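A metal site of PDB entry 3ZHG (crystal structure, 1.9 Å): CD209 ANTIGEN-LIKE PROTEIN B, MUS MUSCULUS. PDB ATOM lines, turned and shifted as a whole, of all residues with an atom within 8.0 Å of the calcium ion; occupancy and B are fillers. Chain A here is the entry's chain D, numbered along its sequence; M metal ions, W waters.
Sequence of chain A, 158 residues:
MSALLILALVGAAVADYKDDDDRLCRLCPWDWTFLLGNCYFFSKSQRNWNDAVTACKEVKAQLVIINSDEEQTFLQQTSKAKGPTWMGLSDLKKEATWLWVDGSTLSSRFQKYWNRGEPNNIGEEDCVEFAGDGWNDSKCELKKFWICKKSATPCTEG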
ATOM      1  N   TRP A  98      -3.852   6.213 -23.084  1.00  0.00           N
ATOM      2  CA  TRP A  98      -4.354   6.927 -21.910  1.00  0.00           C
ATOM      3  C   TRP A  98      -4.881   5.983 -20.849  1.00  0.00           C
ATOM      4  O   TRP A  98      -5.806   5.202 -21.097  1.00  0.00           O
ATOM      5  CB  TRP A  98      -5.421   7.922 -22.312  1.00  0.00           C
ATOM      6  CG  TRP A  98      -4.929   8.912 -23.306  1.00  0.00           C
ATOM      7  CD1 TRP A  98      -4.976   8.811 -24.668  1.00  0.00           C
ATOM      8  CD2 TRP A  98      -4.299  10.167 -23.031  1.00  0.00           C
ATOM      9  NE1 TRP A  98      -4.413   9.917 -25.257  1.00  0.00           N
ATOM     10  CE2 TRP A  98      -3.989  10.773 -24.270  1.00  0.00           C
ATOM     11  CE3 TRP A  98      -3.943  10.834 -21.853  1.00  0.00           C
ATOM     12  CZ2 TRP A  98      -3.363  12.012 -24.366  1.00  0.00           C
ATOM     13  CZ3 TRP A  98      -3.325  12.069 -21.954  1.00  0.00           C
ATOM     14  CH2 TRP A  98      -3.035  12.643 -23.196  1.00  0.00           C
ATOM     15  N   TRP A 114     -13.174  14.209 -25.073  1.00  0.00           N
ATOM     16  CA  TRP A 114     -12.117  14.997 -25.699  1.00  0.00           C
ATOM     17  C   TRP A 114     -12.752  16.145 -26.443  1.00  0.00           C
ATOM     18  O   TRP A 114     -13.700  15.957 -27.188  1.00  0.00           O
ATOM     19  CB  TRP A 114     -11.344  14.169 -26.711  1.00  0.00           C
ATOM     20  CG  TRP A 114     -10.430  13.212 -26.111  1.00  0.00           C
ATOM     21  CD1 TRP A 114     -10.432  11.858 -26.276  1.00  0.00           C
ATOM     22  CD2 TRP A 114      -9.361  13.505 -25.206  1.00  0.00           C
ATOM     23  NE1 TRP A 114      -9.420  11.291 -25.536  1.00  0.00           N
ATOM     24  CE2 TRP A 114      -8.752  12.282 -24.873  1.00  0.00           C
ATOM     25  CE3 TRP A 114      -8.861  14.696 -24.655  1.00  0.00           C
ATOM     26  CZ2 TRP A 114      -7.666  12.215 -24.004  1.00  0.00           C
ATOM     27  CZ3 TRP A 114      -7.786  14.621 -23.804  1.00  0.00           C
ATOM     28  CH2 TRP A 114      -7.189  13.391 -23.488  1.00  0.00           C
ATOM     29  N   GLY A 117      -9.852  18.888 -31.291  1.00  0.00           N
ATOM     30  CA  GLY A 117      -8.496  19.387 -31.318  1.00  0.00           C
ATOM     31  C   GLY A 117      -7.703  18.698 -30.241  1.00  0.00           C
ATOM     32  O   GLY A 117      -6.486  18.859 -30.129  1.00  0.00           O
ATOM     33  N   GLU A 118      -8.397  17.906 -29.431  1.00  0.00           N
ATOM     34  CA  GLU A 118      -7.750  17.171 -28.362  1.00  0.00           C
ATOM     35  C   GLU A 118      -8.008  15.678 -28.522  1.00  0.00           C
ATOM     36  O   GLU A 118      -9.065  15.275 -29.021  1.00  0.00           O
ATOM     37  CB  GLU A 118      -8.270  17.662 -27.013  1.00  0.00           C
ATOM     38  CG  GLU A 118      -8.135  19.156 -26.834  1.00  0.00           C
ATOM     39  CD  GLU A 118      -6.746  19.585 -26.373  1.00  0.00           C
ATOM     40  OE1 GLU A 118      -5.911  18.696 -26.059  1.00  0.00           O
ATOM     41  OE2 GLU A 118      -6.494  20.799 -26.329  1.00  0.00           O
ATOM     42  N   PRO A 119      -7.041  14.857 -28.125  1.00  0.00           N
ATOM     43  CA  PRO A 119      -5.748  15.337 -27.604  1.00  0.00           C
ATOM     44  C   PRO A 119      -4.752  15.675 -28.703  1.00  0.00           C
ATOM     45  O   PRO A 119      -4.643  14.923 -29.668  1.00  0.00           O
ATOM     46  CB  PRO A 119      -5.232  14.127 -26.812  1.00  0.00           C
ATOM     47  CG  PRO A 119      -5.831  12.954 -27.520  1.00  0.00           C
ATOM     48  CD  PRO A 119      -7.180  13.392 -28.001  1.00  0.00           C
ATOM     49  N   ASN A 120      -4.049  16.797 -28.554  1.00  0.00           N
ATOM     50  CA  ASN A 120      -2.948  17.158 -29.455  1.00  0.00           C
ATOM     51  C   ASN A 120      -1.607  17.173 -28.721  1.00  0.00           C
ATOM     52  O   ASN A 120      -1.505  16.621 -27.625  1.00  0.00           O
ATOM     53  CB  ASN A 120      -3.204  18.525 -30.092  1.00  0.00           C
ATOM     54  CG  ASN A 120      -3.282  19.617 -29.071  1.00  0.00           C
ATOM     55  OD1 ASN A 120      -3.043  19.390 -27.891  1.00  0.00           O
ATOM     56  ND2 ASN A 120      -3.610  20.826 -29.517  1.00  0.00           N
ATOM     57  N   ASN A 121      -0.594  17.812 -29.308  1.00  0.00           N
ATOM     58  CA  ASN A 121       0.734  17.886 -28.697  1.00  0.00           C
ATOM     59  C   ASN A 121       1.163  16.595 -27.989  1.00  0.00           C
ATOM     60  O   ASN A 121       1.673  16.620 -26.861  1.00  0.00           O
ATOM     61  CB  ASN A 121       0.791  19.048 -27.714  1.00  0.00           C
ATOM     62  CG  ASN A 121       0.590  20.379 -28.396  1.00  0.00           C
ATOM     63  OD1 ASN A 121       1.132  20.622 -29.468  1.00  0.00           O
ATOM     64  ND2 ASN A 121      -0.187  21.256 -27.769  1.00  0.00           N
ATOM     65  N   ILE A 122       0.950  15.470 -28.652  1.00  0.00           N
ATOM     66  CA  ILE A 122       1.190  14.159 -28.060  1.00  0.00           C
ATOM     67  C   ILE A 122       2.635  14.003 -27.632  1.00  0.00           C
ATOM     68  O   ILE A 122       3.555  14.421 -28.345  1.00  0.00           O
ATOM     69  CB  ILE A 122       0.805  13.025 -29.017  1.00  0.00           C
ATOM     70  CG1 ILE A 122      -0.660  13.162 -29.435  1.00  0.00           C
ATOM     71  CG2 ILE A 122       1.028  11.667 -28.373  1.00  0.00           C
ATOM     72  CD1 ILE A 122      -1.634  12.743 -28.368  1.00  0.00           C
ATOM     73  N   GLU A 124       4.077  15.615 -25.508  1.00  0.00           N
ATOM     74  CA  GLU A 124       4.434  16.854 -24.807  1.00  0.00           C
ATOM     75  C   GLU A 124       3.439  17.161 -23.674  1.00  0.00           C
ATOM     76  O   GLU A 124       3.845  17.491 -22.547  1.00  0.00           O
ATOM     77  CB  GLU A 124       4.487  18.018 -25.801  1.00  0.00           C
ATOM     78  CG  GLU A 124       4.563  19.378 -25.131  1.00  0.00           C
ATOM     79  CD  GLU A 124       4.128  20.513 -26.049  1.00  0.00           C
ATOM     80  OE1 GLU A 124       4.618  20.557 -27.204  1.00  0.00           O
ATOM     81  OE2 GLU A 124       3.292  21.353 -25.623  1.00  0.00           O
ATOM     82  N   GLU A 125       2.149  17.079 -23.978  1.00  0.00           N
ATOM     83  CA  GLU A 125       1.105  17.316 -22.988  1.00  0.00           C
ATOM     84  C   GLU A 125       0.464  16.001 -22.585  1.00  0.00           C
ATOM     85  O   GLU A 125      -0.396  15.481 -23.294  1.00  0.00           O
ATOM     86  CB  GLU A 125       0.047  18.255 -23.560  1.00  0.00           C
ATOM     87  CG  GLU A 125       0.540  19.676 -23.765  1.00  0.00           C
ATOM     88  CD  GLU A 125      -0.503  20.557 -24.425  1.00  0.00           C
ATOM     89  OE1 GLU A 125      -1.387  20.017 -25.115  1.00  0.00           O
ATOM     90  OE2 GLU A 125      -0.434  21.799 -24.253  1.00  0.00           O
ATOM     91  N   ASP A 126       0.894  15.471 -21.450  1.00  0.00           N
ATOM     92  CA  ASP A 126       0.589  14.097 -21.083  1.00  0.00           C
ATOM     93  C   ASP A 126      -0.493  13.925 -20.027  1.00  0.00           C
ATOM     94  O   ASP A 126      -0.853  12.799 -19.678  1.00  0.00           O
ATOM     95  CB  ASP A 126       1.871  13.407 -20.608  1.00  0.00           C
ATOM     96  CG  ASP A 126       2.916  13.315 -21.692  1.00  0.00           C
ATOM     97  OD1 ASP A 126       2.650  12.608 -22.697  1.00  0.00           O
ATOM     98  OD2 ASP A 126       3.992  13.945 -21.557  1.00  0.00           O
ATOM     99  N   CYS A 127      -1.023  15.035 -19.522  1.00  0.00           N
ATOM    100  CA  CYS A 127      -2.001  14.969 -18.436  1.00  0.00           C
ATOM    101  C   CYS A 127      -3.328  15.567 -18.855  1.00  0.00           C
ATOM    102  O   CYS A 127      -3.368  16.521 -19.639  1.00  0.00           O
ATOM    103  CB  CYS A 127      -1.451  15.666 -17.185  1.00  0.00           C
ATOM    104  SG  CYS A 127      -0.089  14.766 -16.407  1.00  0.00           S
ATOM    105  N   GLU A 129      -7.129  17.362 -18.349  1.00  0.00           N
ATOM    106  CA  GLU A 129      -7.841  18.331 -17.536  1.00  0.00           C
ATOM    107  C   GLU A 129      -9.260  18.503 -18.027  1.00  0.00           C
ATOM    108  O   GLU A 129      -9.543  18.279 -19.205  1.00  0.00           O
ATOM    109  CB  GLU A 129      -7.155  19.685 -17.645  1.00  0.00           C
ATOM    110  CG  GLU A 129      -7.328  20.321 -19.011  1.00  0.00           C
ATOM    111  CD  GLU A 129      -6.794  21.743 -19.063  1.00  0.00           C
ATOM    112  OE1 GLU A 129      -6.459  22.301 -17.998  1.00  0.00           O
ATOM    113  OE2 GLU A 129      -6.683  22.304 -20.169  1.00  0.00           O
ATOM    114  N   TRP A 135     -12.561  17.733 -22.445  1.00  0.00           N
ATOM    115  CA  TRP A 135     -11.226  17.366 -21.962  1.00  0.00           C
ATOM    116  C   TRP A 135     -10.085  17.833 -22.876  1.00  0.00           C
ATOM    117  O   TRP A 135     -10.135  17.625 -24.085  1.00  0.00           O
ATOM    118  CB  TRP A 135     -11.102  15.843 -21.853  1.00  0.00           C
ATOM    119  CG  TRP A 135     -12.105  15.193 -20.973  1.00  0.00           C
ATOM    120  CD1 TRP A 135     -13.058  15.803 -20.207  1.00  0.00           C
ATOM    121  CD2 TRP A 135     -12.259  13.774 -20.751  1.00  0.00           C
ATOM    122  NE1 TRP A 135     -13.787  14.861 -19.533  1.00  0.00           N
ATOM    123  CE2 TRP A 135     -13.317  13.620 -19.848  1.00  0.00           C
ATOM    124  CE3 TRP A 135     -11.594  12.650 -21.238  1.00  0.00           C
ATOM    125  CZ2 TRP A 135     -13.744  12.363 -19.413  1.00  0.00           C
ATOM    126  CZ3 TRP A 135     -12.025  11.412 -20.813  1.00  0.00           C
ATOM    127  CH2 TRP A 135     -13.079  11.271 -19.907  1.00  0.00           C
ATOM    128  N   ASN A 136      -9.065  18.439 -22.269  1.00  0.00           N
ATOM    129  CA  ASN A 136      -7.797  18.711 -22.956  1.00  0.00           C
ATOM    130  C   ASN A 136      -6.711  17.806 -22.401  1.00  0.00           C
ATOM    131  O   ASN A 136      -6.816  17.362 -21.256  1.00  0.00           O
ATOM    132  CB  ASN A 136      -7.344  20.145 -22.732  1.00  0.00           C
ATOM    133  CG  ASN A 136      -8.182  21.148 -23.447  1.00  0.00           C
ATOM    134  OD1 ASN A 136      -9.117  20.793 -24.150  1.00  0.00           O
ATOM    135  ND2 ASN A 136      -7.874  22.423 -23.268  1.00  0.00           N
ATOM    136  N   ASP A 137      -5.684  17.537 -23.191  1.00  0.00           N
ATOM    137  CA  ASP A 137      -4.436  17.097 -22.590  1.00  0.00           C
ATOM    138  C   ASP A 137      -3.601  18.353 -22.373  1.00  0.00           C
ATOM    139  O   ASP A 137      -3.736  19.323 -23.112  1.00  0.00           O
ATOM    140  CB  ASP A 137      -3.706  16.036 -23.418  1.00  0.00           C
ATOM    141  CG  ASP A 137      -3.286  16.546 -24.794  1.00  0.00           C
ATOM    142  OD1 ASP A 137      -3.563  17.710 -25.154  1.00  0.00           O
ATOM    143  OD2 ASP A 137      -2.659  15.736 -25.507  1.00  0.00           O
ATOM    144  N   SER A 138      -2.782  18.347 -21.323  1.00  0.00           N
ATOM    145  CA  SER A 138      -2.061  19.555 -20.943  1.00  0.00           C
ATOM    146  C   SER A 138      -0.725  19.204 -20.312  1.00  0.00           C
ATOM    147  O   SER A 138      -0.515  18.070 -19.903  1.00  0.00           O
ATOM    148  CB  SER A 138      -2.926  20.379 -19.986  1.00  0.00           C
ATOM    149  OG  SER A 138      -2.595  21.749 -20.074  1.00  0.00           O
ATOM    150  N   LYS A 139       0.190  20.182 -20.257  1.00  0.00           N
ATOM    151  CA  LYS A 139       1.491  20.004 -19.611  1.00  0.00           C
ATOM    152  C   LYS A 139       1.348  19.687 -18.123  1.00  0.00           C
ATOM    153  O   LYS A 139       0.879  20.510 -17.345  1.00  0.00           O
ATOM    154  CB  LYS A 139       2.356  21.246 -19.782  1.00  0.00           C
ATOM    155  CG  LYS A 139       3.087  21.328 -21.118  1.00  0.00           C
ATOM    156  CD  LYS A 139       3.585  22.745 -21.399  1.00  0.00           C
ATOM    157  CE  LYS A 139       2.424  23.743 -21.443  1.00  0.00           C
ATOM    158  NZ  LYS A 139       2.805  25.053 -22.028  1.00  0.00           N
HETATM  159 CA    CA M   1      -3.760  19.955 -25.556  1.00  0.00          CA
HETATM  160  O   HOH W   1      -4.510  22.427 -26.006  1.00  0.00           O
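The side-chain amide nitrogen (ND2) of Asn 121 lies close to the side-chain carboxylate (OE1) of Glu 125 (3.2 Å).
ND2 of Asn 121 sits close to OD1 of Asn 120, 3.4 Å away.
The side-chain carboxylate (OE2) of Glu 118 sits close to the side-chain amide oxygen (OD1) of Asn 136 (3.4 Å).
Of the 18 residues printed, 4 come within 4 Å of the calcium ion.
The calcium ion is bound by OD1 of Asp 137 (2.3 Å), OE1 of Glu 125 (2.4 Å), OD1 of Asn 120 (2.5 Å), O of Asp 137 (2.5 Å), OE1 of Glu 118 (2.5 Å) and water W1 (2.6 Å).
The calcium ion has six donor atoms within binding distance.
Slightly farther from the calcium ion lies OE2 of Glu 118 (3.0 Å).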
